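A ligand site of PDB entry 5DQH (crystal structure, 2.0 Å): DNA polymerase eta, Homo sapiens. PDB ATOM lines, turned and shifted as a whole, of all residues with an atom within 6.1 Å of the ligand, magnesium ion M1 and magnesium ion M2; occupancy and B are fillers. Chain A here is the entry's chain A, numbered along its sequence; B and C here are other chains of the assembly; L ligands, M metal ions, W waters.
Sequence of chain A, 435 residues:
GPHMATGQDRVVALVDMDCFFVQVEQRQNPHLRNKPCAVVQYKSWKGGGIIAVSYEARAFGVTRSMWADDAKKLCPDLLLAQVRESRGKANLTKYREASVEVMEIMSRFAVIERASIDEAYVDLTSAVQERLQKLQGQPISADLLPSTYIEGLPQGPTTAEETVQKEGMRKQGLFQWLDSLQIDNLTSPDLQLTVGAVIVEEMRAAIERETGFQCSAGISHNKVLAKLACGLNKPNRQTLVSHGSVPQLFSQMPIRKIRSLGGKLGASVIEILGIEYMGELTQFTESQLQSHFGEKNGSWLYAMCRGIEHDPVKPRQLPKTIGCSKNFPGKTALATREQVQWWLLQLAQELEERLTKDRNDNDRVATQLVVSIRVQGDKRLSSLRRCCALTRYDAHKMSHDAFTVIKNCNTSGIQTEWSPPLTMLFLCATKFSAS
The backbone NH (N) of Cys 19 is in hydrogen-bond range of an oxygen (O7) of the ligand, 2.9 Å away. N of Phe 20 lies within hydrogen-bond range of O6 of the ligand (3.3 Å). The backbone NH (N) of Phe 21 lies within hydrogen-bond range of an oxygen (O8) of the ligand (3.1 Å). The side-chain hydroxyl (OH) of Tyr 55 lies within hydrogen-bond range of an oxygen (O7) of the ligand (2.7 Å). O2 of 5EJ 4 of chain C lies within hydrogen-bond range of a nitrogen (N1) of the ligand, at 2.5 Å. O4' of DA 5 of chain C is in hydrogen-bond range of a nitrogen (N2) of the ligand, at 3.1 Å. NE2 of Gln 41 sits close to N2 of the ligand, at 3.3 Å. The side-chain amino group (NZ) of Lys 234 lies within salt-bridge range of an oxygen (O7) of the ligand (3.0 Å). The guanidinium group (NH2) of Arg 58 lies within salt-bridge range of an oxygen (O10) of the ligand, 3.2 Å away.
OG of Ser 116 is in hydrogen-bond range of N of Glu 119. The side-chain hydroxyl (OG) of Ser 116 lies close to the backbone NH (N) of Asp 118 (3.1 Å). O2 of 5EJ 4 of chain C lies within hydrogen-bond range of the side-chain amide nitrogen (NE2) of Gln 41, 2.8 Å away. The backbone carbonyl oxygen (O) of Met 17 sits close to the side-chain amino group (NZ) of Lys 234. The backbone carbonyl oxygen (O) of Asp 16 is in hydrogen-bond range of the backbone NH (N) of Ser 216. The side-chain hydroxyl of Ser 116 lies close to O3' of DT 8 of chain B (3.4 Å). OG of Ser 216 sits at hydrogen-bond distance from OD1 of Asp 18, at 2.8 Å. The side-chain carboxylate (OD1) of Asp 18 lies within salt-bridge range of the side-chain amino group (NZ) of Lys 234 (2.8 Å).
CA of Asp 18 touches O7 of the ligand, 3.2 Å away. Ile 51 touches the ligand (O to C7, 3.5 Å). Ala 52 touches the ligand (CB to O8, 3.6 Å). CG2 of Ile 117 touches O11 of the ligand, at 3.7 Å. Within 4 Å of the ligand: Asp 16, Met 17, Asp 18, Cys 19, Phe 20, Phe 21, Gln 41, Ile 51, Ala 52, Tyr 55, Arg 58, Ile 117, Asp 118, Lys 234, DT 8 of chain B, 5EJ 4 of chain C and DA 5 of chain C. Along chain A the residues within 4 Å of the ligand span positions 16 to 234.
Ser 116 touches magnesium ion M1 (OG to MG, 3.8 Å).
Lys 234 touches magnesium ion M2 (NZ to MG, 3.9 Å). Four residues have an atom within 4 Å of magnesium ion M2: Asp 16, Met 17, Asp 118 and Lys 234. The nearest printed residue that does not touch magnesium ion M2 is Asp 18 (4.4 Å).
Magnesium ion M1 is bound by the side-chain carboxylate (OD1) of Asp 118 (2.0 Å), the side-chain carboxylate (OE2) of Glu 119 (2.1 Å), O3' of DT 8 of chain B (2.1 Å), an oxygen (O2) of the ligand (2.1 Å), the side-chain carboxylate (OD1) of Asp 16 (2.2 Å) and water W2 (2.2 Å). Magnesium ion M1 has six donor atoms within binding distance.
Magnesium ion M2 is bound by O3 of the ligand (2.0 Å), O4 of the ligand (2.1 Å), OD2 of Asp 118 (2.1 Å), OD2 of Asp 16 (2.1 Å), O of Met 17 (2.2 Å) and O2 of the ligand (2.2 Å).
Water W2 bridges NZ of Lys 227 (3.0 Å) and O5 of the ligand (3.1 Å). Water W3 lies within hydrogen-bond range of O6 of the ligand (2.6 Å), NH2 of Arg 58 (2.9 Å) and N of Val 53 (2.9 Å). Water W5 lies within hydrogen-bond range of the backbone carbonyl oxygen (O) of Ile 51 (2.8 Å), the guanidinium group (NE) of Arg 64 (3.3 Å) and a nitrogen (N6) of the ligand (3.3 Å). Water W1 bridges O2 of DT 8 of chain B (2.7 Å) and an oxygen (O11) of the ligand (3.4 Å).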
ATOM      1  N   ASP A  16       8.901  27.568 -10.573  1.00  0.00           N
ATOM      2  CA  ASP A  16       9.369  27.135 -11.877  1.00  0.00           C
ATOM      3  C   ASP A  16      10.717  27.749 -12.305  1.00  0.00           C
ATOM      4  O   ASP A  16      10.859  28.973 -12.345  1.00  0.00           O
ATOM      5  CB  ASP A  16       8.301  27.437 -12.927  1.00  0.00           C
ATOM      6  CG  ASP A  16       8.599  26.788 -14.237  1.00  0.00           C
ATOM      7  OD1 ASP A  16       8.071  25.675 -14.500  1.00  0.00           O
ATOM      8  OD2 ASP A  16       9.383  27.367 -14.991  1.00  0.00           O
ATOM      9  N   MET A  17      11.698  26.910 -12.639  1.00  0.00           N
ATOM     10  CA  MET A  17      13.011  27.409 -13.033  1.00  0.00           C
ATOM     11  C   MET A  17      12.890  28.224 -14.334  1.00  0.00           C
ATOM     12  O   MET A  17      12.151  27.861 -15.245  1.00  0.00           O
ATOM     13  CB  MET A  17      14.009  26.260 -13.213  1.00  0.00           C
ATOM     14  CG  MET A  17      13.992  25.244 -12.066  1.00  0.00           C
ATOM     15  SD  MET A  17      14.242  26.042 -10.449  1.00  0.00           S
ATOM     16  CE  MET A  17      15.824  26.800 -10.726  1.00  0.00           C
ATOM     17  N   ASP A  18      13.579  29.352 -14.388  1.00  0.00           N
ATOM     18  CA  ASP A  18      13.624  30.171 -15.590  1.00  0.00           C
ATOM     19  C   ASP A  18      14.524  29.479 -16.617  1.00  0.00           C
ATOM     20  O   ASP A  18      15.599  29.019 -16.251  1.00  0.00           O
ATOM     21  CB  ASP A  18      14.162  31.564 -15.268  1.00  0.00           C
ATOM     22  CG  ASP A  18      13.253  32.353 -14.290  1.00  0.00           C
ATOM     23  OD1 ASP A  18      12.042  32.125 -14.278  1.00  0.00           O
ATOM     24  OD2 ASP A  18      13.775  33.223 -13.559  1.00  0.00           O
ATOM     25  N   CYS A  19      14.076  29.431 -17.882  1.00  0.00           N
ATOM     26  CA  CYS A  19      14.762  28.761 -19.008  1.00  0.00           C
ATOM     27  C   CYS A  19      15.712  27.665 -18.527  1.00  0.00           C
ATOM     28  O   CYS A  19      16.926  27.783 -18.676  1.00  0.00           O
ATOM     29  CB  CYS A  19      15.526  29.795 -19.882  1.00  0.00           C
ATOM     30  SG  CYS A  19      16.559  31.003 -19.008  1.00  0.00           S
ATOM     31  N   PHE A  20      15.146  26.633 -17.917  1.00  0.00           N
ATOM     32  CA  PHE A  20      15.942  25.746 -17.042  1.00  0.00           C
ATOM     33  C   PHE A  20      17.178  25.113 -17.718  1.00  0.00           C
ATOM     34  O   PHE A  20      18.300  25.251 -17.204  1.00  0.00           O
ATOM     35  CB  PHE A  20      15.054  24.650 -16.455  1.00  0.00           C
ATOM     36  CG  PHE A  20      15.759  23.780 -15.439  1.00  0.00           C
ATOM     37  CD1 PHE A  20      16.536  24.339 -14.439  1.00  0.00           C
ATOM     38  CD2 PHE A  20      15.642  22.391 -15.492  1.00  0.00           C
ATOM     39  CE1 PHE A  20      17.195  23.538 -13.507  1.00  0.00           C
ATOM     40  CE2 PHE A  20      16.302  21.583 -14.553  1.00  0.00           C
ATOM     41  CZ  PHE A  20      17.067  22.156 -13.566  1.00  0.00           C
ATOM     42  N   PHE A  21      17.001  24.438 -18.860  1.00  0.00           N
ATOM     43  CA  PHE A  21      18.151  23.739 -19.455  1.00  0.00           C
ATOM     44  C   PHE A  21      19.232  24.759 -19.843  1.00  0.00           C
ATOM     45  O   PHE A  21      20.416  24.470 -19.747  1.00  0.00           O
ATOM     46  CB  PHE A  21      17.747  22.902 -20.683  1.00  0.00           C
ATOM     47  CG  PHE A  21      16.953  21.673 -20.365  1.00  0.00           C
ATOM     48  CD1 PHE A  21      16.357  21.499 -19.133  1.00  0.00           C
ATOM     49  CD2 PHE A  21      16.796  20.675 -21.324  1.00  0.00           C
ATOM     50  CE1 PHE A  21      15.606  20.363 -18.856  1.00  0.00           C
ATOM     51  CE2 PHE A  21      16.054  19.525 -21.047  1.00  0.00           C
ATOM     52  CZ  PHE A  21      15.460  19.372 -19.810  1.00  0.00           C
ATOM     53  N   VAL A  22      18.820  25.948 -20.290  1.00  0.00           N
ATOM     54  CA  VAL A  22      19.767  27.013 -20.576  1.00  0.00           C
ATOM     55  C   VAL A  22      20.575  27.445 -19.343  1.00  0.00           C
ATOM     56  O   VAL A  22      21.790  27.624 -19.438  1.00  0.00           O
ATOM     57  CB  VAL A  22      19.056  28.255 -21.171  1.00  0.00           C
ATOM     58  CG1 VAL A  22      19.985  29.446 -21.212  1.00  0.00           C
ATOM     59  CG2 VAL A  22      18.548  27.952 -22.590  1.00  0.00           C
ATOM     60  N   GLN A  41      18.473  19.822 -29.338  1.00  0.00           N
ATOM     61  CA  GLN A  41      18.891  18.425 -29.393  1.00  0.00           C
ATOM     62  C   GLN A  41      19.078  17.987 -30.829  1.00  0.00           C
ATOM     63  O   GLN A  41      18.332  18.406 -31.732  1.00  0.00           O
ATOM     64  CB  GLN A  41      17.917  17.496 -28.640  1.00  0.00           C
ATOM     65  CG  GLN A  41      16.508  17.962 -28.552  1.00  0.00           C
ATOM     66  CD  GLN A  41      15.655  17.095 -27.619  1.00  0.00           C
ATOM     67  OE1 GLN A  41      16.147  16.462 -26.674  1.00  0.00           O
ATOM     68  NE2 GLN A  41      14.360  17.071 -27.901  1.00  0.00           N
ATOM     69  N   ILE A  51      14.840  23.465 -27.488  1.00  0.00           N
ATOM     70  CA  ILE A  51      13.906  23.132 -26.414  1.00  0.00           C
ATOM     71  C   ILE A  51      13.961  24.070 -25.208  1.00  0.00           C
ATOM     72  O   ILE A  51      13.080  24.002 -24.343  1.00  0.00           O
ATOM     73  CB  ILE A  51      14.090  21.691 -25.933  1.00  0.00           C
ATOM     74  CG1 ILE A  51      15.502  21.462 -25.386  1.00  0.00           C
ATOM     75  CG2 ILE A  51      13.758  20.700 -27.061  1.00  0.00           C
ATOM     76  CD1 ILE A  51      15.637  20.102 -24.710  1.00  0.00           C
ATOM     77  N   ALA A  52      14.959  24.950 -25.153  1.00  0.00           N
ATOM     78  CA  ALA A  52      15.000  25.990 -24.109  1.00  0.00           C
ATOM     79  C   ALA A  52      15.654  27.255 -24.652  1.00  0.00           C
ATOM     80  O   ALA A  52      16.595  27.168 -25.429  1.00  0.00           O
ATOM     81  CB  ALA A  52      15.745  25.489 -22.865  1.00  0.00           C
ATOM     82  N   VAL A  53      15.179  28.422 -24.210  1.00  0.00           N
ATOM     83  CA  VAL A  53      15.603  29.685 -24.807  1.00  0.00           C
ATOM     84  C   VAL A  53      15.834  30.737 -23.712  1.00  0.00           C
ATOM     85  O   VAL A  53      14.929  30.959 -22.898  1.00  0.00           O
ATOM     86  CB  VAL A  53      14.549  30.231 -25.818  1.00  0.00           C
ATOM     87  CG1 VAL A  53      15.079  31.433 -26.569  1.00  0.00           C
ATOM     88  CG2 VAL A  53      14.142  29.172 -26.788  1.00  0.00           C
ATOM     89  N   TYR A  55      16.144  34.415 -21.914  1.00  0.00           N
ATOM     90  CA  TYR A  55      15.257  35.563 -22.114  1.00  0.00           C
ATOM     91  C   TYR A  55      15.846  36.596 -23.085  1.00  0.00           C
ATOM     92  O   TYR A  55      15.113  37.248 -23.796  1.00  0.00           O
ATOM     93  CB  TYR A  55      14.891  36.199 -20.773  1.00  0.00           C
ATOM     94  CG  TYR A  55      13.818  35.354 -20.125  1.00  0.00           C
ATOM     95  CD1 TYR A  55      14.121  34.117 -19.552  1.00  0.00           C
ATOM     96  CD2 TYR A  55      12.474  35.734 -20.183  1.00  0.00           C
ATOM     97  CE1 TYR A  55      13.130  33.310 -18.998  1.00  0.00           C
ATOM     98  CE2 TYR A  55      11.474  34.942 -19.628  1.00  0.00           C
ATOM     99  CZ  TYR A  55      11.801  33.726 -19.039  1.00  0.00           C
ATOM    100  OH  TYR A  55      10.800  32.940 -18.491  1.00  0.00           O
ATOM    101  N   ARG A  58      14.862  35.172 -26.469  1.00  0.00           N
ATOM    102  CA  ARG A  58      13.404  35.352 -26.656  1.00  0.00           C
ATOM    103  C   ARG A  58      13.070  36.751 -27.178  1.00  0.00           C
ATOM    104  O   ARG A  58      12.110  36.918 -27.941  1.00  0.00           O
ATOM    105  CB  ARG A  58      12.650  35.116 -25.348  1.00  0.00           C
ATOM    106  CG  ARG A  58      12.858  33.760 -24.740  1.00  0.00           C
ATOM    107  CD  ARG A  58      11.938  33.535 -23.546  1.00  0.00           C
ATOM    108  NE  ARG A  58      12.289  32.297 -22.843  1.00  0.00           N
ATOM    109  CZ  ARG A  58      11.562  31.728 -21.897  1.00  0.00           C
ATOM    110  NH1 ARG A  58      10.412  32.276 -21.514  1.00  0.00           N
ATOM    111  NH2 ARG A  58      11.981  30.595 -21.347  1.00  0.00           N
ATOM    112  N   ARG A  64      10.959  27.892 -28.251  1.00  0.00           N
ATOM    113  CA  ARG A  64      10.876  26.435 -28.232  1.00  0.00           C
ATOM    114  C   ARG A  64      10.312  25.895 -29.550  1.00  0.00           C
ATOM    115  O   ARG A  64       9.443  26.537 -30.142  1.00  0.00           O
ATOM    116  CB  ARG A  64       9.985  25.978 -27.070  1.00  0.00           C
ATOM    117  CG  ARG A  64       9.870  24.479 -26.887  1.00  0.00           C
ATOM    118  CD  ARG A  64       8.568  24.081 -26.179  1.00  0.00           C
ATOM    119  NE  ARG A  64       8.305  24.882 -24.991  1.00  0.00           N
ATOM    120  CZ  ARG A  64       7.389  25.840 -24.917  1.00  0.00           C
ATOM    121  NH1 ARG A  64       6.643  26.134 -25.969  1.00  0.00           N
ATOM    122  NH2 ARG A  64       7.210  26.518 -23.791  1.00  0.00           N
ATOM    123  N   LEU A  92      19.251  13.101 -21.114  1.00  0.00           N
ATOM    124  CA  LEU A  92      18.875  14.267 -20.306  1.00  0.00           C
ATOM    125  C   LEU A  92      19.407  14.207 -18.874  1.00  0.00           C
ATOM    126  O   LEU A  92      18.956  14.969 -18.015  1.00  0.00           O
ATOM    127  CB  LEU A  92      17.352  14.424 -20.282  1.00  0.00           C
ATOM    128  CG  LEU A  92      16.687  14.483 -21.652  1.00  0.00           C
ATOM    129  CD1 LEU A  92      15.165  14.436 -21.501  1.00  0.00           C
ATOM    130  CD2 LEU A  92      17.122  15.749 -22.394  1.00  0.00           C
ATOM    131  N   SER A 116       7.241  18.608 -12.897  1.00  0.00           N
ATOM    132  CA  SER A 116       7.969  18.403 -14.137  1.00  0.00           C
ATOM    133  C   SER A 116       9.435  18.420 -13.778  1.00  0.00           C
ATOM    134  O   SER A 116       9.776  18.581 -12.620  1.00  0.00           O
ATOM    135  CB  SER A 116       7.674  19.499 -15.167  1.00  0.00           C
ATOM    136  OG  SER A 116       8.337  20.717 -14.794  1.00  0.00           O
ATOM    137  N   ILE A 117      10.303  18.273 -14.763  1.00  0.00           N
ATOM    138  CA  ILE A 117      11.732  18.377 -14.511  1.00  0.00           C
ATOM    139  C   ILE A 117      12.137  19.732 -13.881  1.00  0.00           C
ATOM    140  O   ILE A 117      13.139  19.800 -13.167  1.00  0.00           O
ATOM    141  CB  ILE A 117      12.543  18.156 -15.798  1.00  0.00           C
ATOM    142  CG1 ILE A 117      13.967  17.690 -15.474  1.00  0.00           C
ATOM    143  CG2 ILE A 117      12.555  19.426 -16.682  1.00  0.00           C
ATOM    144  CD1 ILE A 117      14.694  17.107 -16.726  1.00  0.00           C
ATOM    145  N   ASP A 118      11.370  20.805 -14.115  1.00  0.00           N
ATOM    146  CA  ASP A 118      11.838  22.078 -13.574  1.00  0.00           C
ATOM    147  C   ASP A 118      10.831  22.796 -12.678  1.00  0.00           C
ATOM    148  O   ASP A 118      10.993  23.999 -12.405  1.00  0.00           O
ATOM    149  CB  ASP A 118      12.259  23.026 -14.688  1.00  0.00           C
ATOM    150  CG  ASP A 118      11.121  23.915 -15.165  1.00  0.00           C
ATOM    151  OD1 ASP A 118       9.982  23.418 -15.367  1.00  0.00           O
ATOM    152  OD2 ASP A 118      11.375  25.128 -15.342  1.00  0.00           O
ATOM    153  N   GLU A 119       9.818  22.091 -12.191  1.00  0.00           N
ATOM    154  CA  GLU A 119       8.867  22.776 -11.315  1.00  0.00           C
ATOM    155  C   GLU A 119       8.198  21.850 -10.325  1.00  0.00           C
ATOM    156  O   GLU A 119       8.052  20.649 -10.558  1.00  0.00           O
ATOM    157  CB  GLU A 119       7.822  23.512 -12.146  1.00  0.00           C
ATOM    158  CG  GLU A 119       6.709  22.668 -12.695  1.00  0.00           C
ATOM    159  CD  GLU A 119       6.240  23.208 -14.016  1.00  0.00           C
ATOM    160  OE1 GLU A 119       5.097  23.743 -14.097  1.00  0.00           O
ATOM    161  OE2 GLU A 119       7.013  23.105 -14.983  1.00  0.00           O
ATOM    162  N   SER A 216      11.090  31.569 -11.026  1.00  0.00           N
ATOM    163  CA  SER A 216       9.941  32.410 -10.733  1.00  0.00           C
ATOM    164  C   SER A 216       8.989  31.593  -9.883  1.00  0.00           C
ATOM    165  O   SER A 216       9.161  30.381  -9.772  1.00  0.00           O
ATOM    166  CB  SER A 216       9.291  32.901 -12.018  1.00  0.00           C
ATOM    167  OG  SER A 216      10.238  33.646 -12.785  1.00  0.00           O
ATOM    168  N   LYS A 227       0.087  28.308 -10.469  1.00  0.00           N
ATOM    169  CA  LYS A 227       0.755  28.081 -11.764  1.00  0.00           C
ATOM    170  C   LYS A 227       0.500  29.260 -12.697  1.00  0.00           C
ATOM    171  O   LYS A 227       1.430  29.736 -13.365  1.00  0.00           O
ATOM    172  CB  LYS A 227       0.272  26.760 -12.399  1.00  0.00           C
ATOM    173  CG  LYS A 227       0.816  26.469 -13.823  1.00  0.00           C
ATOM    174  CD  LYS A 227       2.358  26.290 -13.841  1.00  0.00           C
ATOM    175  CE  LYS A 227       2.877  26.098 -15.282  1.00  0.00           C
ATOM    176  NZ  LYS A 227       4.371  26.014 -15.414  1.00  0.00           N
ATOM    177  N   LYS A 234       7.543  36.343 -14.998  1.00  0.00           N
ATOM    178  CA  LYS A 234       8.848  35.765 -15.336  1.00  0.00           C
ATOM    179  C   LYS A 234       9.700  36.757 -16.134  1.00  0.00           C
ATOM    180  O   LYS A 234       9.155  37.556 -16.888  1.00  0.00           O
ATOM    181  CB  LYS A 234       8.647  34.469 -16.142  1.00  0.00           C
ATOM    182  CG  LYS A 234       8.268  33.249 -15.310  1.00  0.00           C
ATOM    183  CD  LYS A 234       8.369  31.939 -16.120  1.00  0.00           C
ATOM    184  CE  LYS A 234       8.634  30.700 -15.227  1.00  0.00           C
ATOM    185  NZ  LYS A 234      10.110  30.316 -15.087  1.00  0.00           N
ATOM    186  N   PRO A 235      11.051  36.702 -15.990  1.00  0.00           N
ATOM    187  CA  PRO A 235      11.879  35.802 -15.169  1.00  0.00           C
ATOM    188  C   PRO A 235      12.261  36.374 -13.799  1.00  0.00           C
ATOM    189  O   PRO A 235      12.164  37.576 -13.576  1.00  0.00           O
ATOM    190  CB  PRO A 235      13.152  35.666 -16.010  1.00  0.00           C
ATOM    191  CG  PRO A 235      13.326  37.081 -16.525  1.00  0.00           C
ATOM    192  CD  PRO A 235      11.904  37.554 -16.843  1.00  0.00           C
ATOM    193  P    DT B   8       2.867  23.582 -19.663  1.00  0.00           P
ATOM    194  OP1  DT B   8       2.826  24.772 -18.789  1.00  0.00           O
ATOM    195  OP2  DT B   8       2.896  23.749 -21.130  1.00  0.00           O
ATOM    196  O5'  DT B   8       4.143  22.655 -19.267  1.00  0.00           O
ATOM    197  C5'  DT B   8       4.470  22.217 -17.862  1.00  0.00           C
ATOM    198  C4'  DT B   8       5.866  21.593 -17.874  1.00  0.00           C
ATOM    199  O4'  DT B   8       5.800  20.544 -18.871  1.00  0.00           O
ATOM    200  C3'  DT B   8       6.860  22.638 -18.394  1.00  0.00           C
ATOM    201  O3'  DT B   8       8.004  22.714 -17.536  1.00  0.00           O
ATOM    202  C2'  DT B   8       7.197  22.168 -19.828  1.00  0.00           C
ATOM    203  C1'  DT B   8       6.861  20.680 -19.793  1.00  0.00           C
ATOM    204  N1   DT B   8       6.435  20.122 -21.122  1.00  0.00           N
ATOM    205  C2   DT B   8       7.101  19.023 -21.624  1.00  0.00           C
ATOM    206  O2   DT B   8       8.015  18.482 -21.052  1.00  0.00           O
ATOM    207  N3   DT B   8       6.639  18.568 -22.833  1.00  0.00           N
ATOM    208  C4   DT B   8       5.599  19.090 -23.572  1.00  0.00           C
ATOM    209  O4   DT B   8       5.265  18.609 -24.640  1.00  0.00           O
ATOM    210  C5   DT B   8       4.949  20.251 -22.990  1.00  0.00           C
ATOM    211  C7   DT B   8       3.809  20.909 -23.724  1.00  0.00           C
ATOM    212  C6   DT B   8       5.397  20.705 -21.808  1.00  0.00           C
ATOM    213  C1  5EJ C   4       7.117  19.906 -27.885  1.00  0.00           C
ATOM    214  C2  5EJ C   4      10.460  17.243 -28.176  1.00  0.00           C
ATOM    215  P   5EJ C   4      10.813  14.607 -34.525  1.00  0.00           P
ATOM    216  OP1 5EJ C   4      11.288  15.314 -35.773  1.00  0.00           O
ATOM    217  O5' 5EJ C   4      12.061  14.380 -33.540  1.00  0.00           O
ATOM    218  C5' 5EJ C   4      12.776  15.512 -33.032  1.00  0.00           C
ATOM    219  C4' 5EJ C   4      12.968  15.395 -31.535  1.00  0.00           C
ATOM    220  C3' 5EJ C   4      12.579  14.026 -30.993  1.00  0.00           C
ATOM    221  O3' 5EJ C   4      13.618  13.635 -30.112  1.00  0.00           O
ATOM    222  C2' 5EJ C   4      11.333  14.279 -30.170  1.00  0.00           C
ATOM    223  C1' 5EJ C   4      11.589  15.702 -29.709  1.00  0.00           C
ATOM    224  O4' 5EJ C   4      12.155  16.348 -30.845  1.00  0.00           O
ATOM    225  N1  5EJ C   4      10.363  16.380 -29.288  1.00  0.00           N
ATOM    226  C6  5EJ C   4       9.209  16.213 -29.946  1.00  0.00           C
ATOM    227  C5  5EJ C   4       8.066  16.885 -29.507  1.00  0.00           C
ATOM    228  C7  5EJ C   4       6.736  16.721 -30.191  1.00  0.00           C
ATOM    229  C4  5EJ C   4       8.194  17.787 -28.337  1.00  0.00           C
ATOM    230  N3  5EJ C   4       9.378  17.912 -27.731  1.00  0.00           N
ATOM    231  O2  5EJ C   4      11.562  17.374 -27.587  1.00  0.00           O
ATOM    232  O4  5EJ C   4       7.097  18.480 -27.870  1.00  0.00           O
ATOM    233  OP2 5EJ C   4      10.145  13.292 -34.877  1.00  0.00           O
ATOM    234  C3  5EJ C   4       5.975  20.464 -27.067  1.00  0.00           C
ATOM    235  P    DA C   5      13.619  12.162 -29.460  1.00  0.00           P
ATOM    236  OP1  DA C   5      14.998  11.638 -29.584  1.00  0.00           O
ATOM    237  OP2  DA C   5      12.491  11.402 -30.027  1.00  0.00           O
ATOM    238  O5'  DA C   5      13.384  12.448 -27.914  1.00  0.00           O
ATOM    239  C5'  DA C   5      14.399  13.135 -27.177  1.00  0.00           C
ATOM    240  C4'  DA C   5      14.075  13.194 -25.705  1.00  0.00           C
ATOM    241  O4'  DA C   5      12.928  14.064 -25.493  1.00  0.00           O
ATOM    242  C3'  DA C   5      13.698  11.851 -25.087  1.00  0.00           C
ATOM    243  O3'  DA C   5      14.222  11.783 -23.783  1.00  0.00           O
ATOM    244  C2'  DA C   5      12.175  11.901 -25.078  1.00  0.00           C
ATOM    245  C1'  DA C   5      11.927  13.375 -24.779  1.00  0.00           C
ATOM    246  N9   DA C   5      10.649  13.878 -25.241  1.00  0.00           N
ATOM    247  C8   DA C   5      10.001  13.553 -26.403  1.00  0.00           C
ATOM    248  N7   DA C   5       8.857  14.196 -26.563  1.00  0.00           N
ATOM    249  C5   DA C   5       8.768  15.010 -25.444  1.00  0.00           C
ATOM    250  C6   DA C   5       7.797  15.933 -25.009  1.00  0.00           C
ATOM    251  N6   DA C   5       6.695  16.216 -25.689  1.00  0.00           N
ATOM    252  N1   DA C   5       8.016  16.573 -23.835  1.00  0.00           N
ATOM    253  C2   DA C   5       9.137  16.282 -23.151  1.00  0.00           C
ATOM    254  N3   DA C   5      10.114  15.439 -23.448  1.00  0.00           N
ATOM    255  C4   DA C   5       9.866  14.816 -24.619  1.00  0.00           C
HETATM  256  N1  LIG L   1      11.232  18.268 -25.301  1.00  0.00           N
HETATM  257  C1  LIG L   1      12.426  18.072 -24.511  1.00  0.00           C
HETATM  258  N2  LIG L   1      13.421  17.045 -24.785  1.00  0.00           N
HETATM  259  N3  LIG L   1      12.659  18.957 -23.377  1.00  0.00           N
HETATM  260  C2  LIG L   1      11.672  20.035 -23.072  1.00  0.00           C
HETATM  261  C3  LIG L   1      10.550  20.239 -23.779  1.00  0.00           C
HETATM  262  C4  LIG L   1      10.286  19.317 -24.971  1.00  0.00           C
HETATM  263  O1  LIG L   1       9.296  19.497 -25.588  1.00  0.00           O
HETATM  264  N4  LIG L   1       9.884  21.276 -23.251  1.00  0.00           N
HETATM  265  C5  LIG L   1      10.598  21.710 -22.184  1.00  0.00           C
HETATM  266  N5  LIG L   1      11.690  20.922 -22.107  1.00  0.00           N
HETATM  267  P1  LIG L   1       9.540  25.012 -19.055  1.00  0.00           P
HETATM  268  P2  LIG L   1      11.838  26.886 -19.331  1.00  0.00           P
HETATM  269  P3  LIG L   1      10.566  29.311 -18.478  1.00  0.00           P
HETATM  270  C6  LIG L   1      12.649  21.180 -21.077  1.00  0.00           C
HETATM  271  O2  LIG L   1       9.401  25.384 -17.600  1.00  0.00           O
HETATM  272  O3  LIG L   1      12.133  26.422 -17.919  1.00  0.00           O
HETATM  273  O4  LIG L   1       9.942  28.352 -17.507  1.00  0.00           O
HETATM  274  C7  LIG L   1      13.382  22.258 -21.377  1.00  0.00           C
HETATM  275  O5  LIG L   1       8.194  24.939 -19.764  1.00  0.00           O
HETATM  276  O6  LIG L   1      12.944  26.566 -20.324  1.00  0.00           O
HETATM  277  O7  LIG L   1      11.332  30.417 -17.797  1.00  0.00           O
HETATM  278  C8  LIG L   1      12.992  23.383 -20.271  1.00  0.00           C
HETATM  279  O8  LIG L   1      14.156  24.155 -19.975  1.00  0.00           O
HETATM  280  N6  LIG L   1      10.382  26.220 -19.901  1.00  0.00           N
HETATM  281  O9  LIG L   1      11.630  28.494 -19.412  1.00  0.00           O
HETATM  282  O10 LIG L   1       9.525  29.911 -19.415  1.00  0.00           O
HETATM  283  C9  LIG L   1      12.548  22.677 -19.170  1.00  0.00           C
HETATM  284  O11 LIG L   1      11.880  21.439 -19.720  1.00  0.00           O
HETATM  285  C10 LIG L   1      11.481  23.414 -18.359  1.00  0.00           C
HETATM  286  O12 LIG L   1      10.314  23.559 -19.143  1.00  0.00           O
HETATM  287 MG    MG M   1       8.326  24.279 -16.142  1.00  0.00          MG
HETATM  288 MG    MG M   2      10.725  26.754 -16.470  1.00  0.00          MG
HETATM  289  O   HOH W   1      10.473  18.332 -19.999  1.00  0.00           O
HETATM  290  O   HOH W   2       6.714  25.433 -17.142  1.00  0.00           O
HETATM  291  O   HOH W   3      12.846  28.052 -22.451  1.00  0.00           O
HETATM  292  O   HOH W   4       8.712  28.907 -21.484  1.00  0.00           O
HETATM  293  O   HOH W   5      10.985  25.475 -23.100  1.00  0.00           O
HETATM  294  O   HOH W   6       9.687  20.640 -18.254  1.00  0.00           O
HETATM  295  O   HOH W   7       7.383  28.014 -17.371  1.00  0.00           O
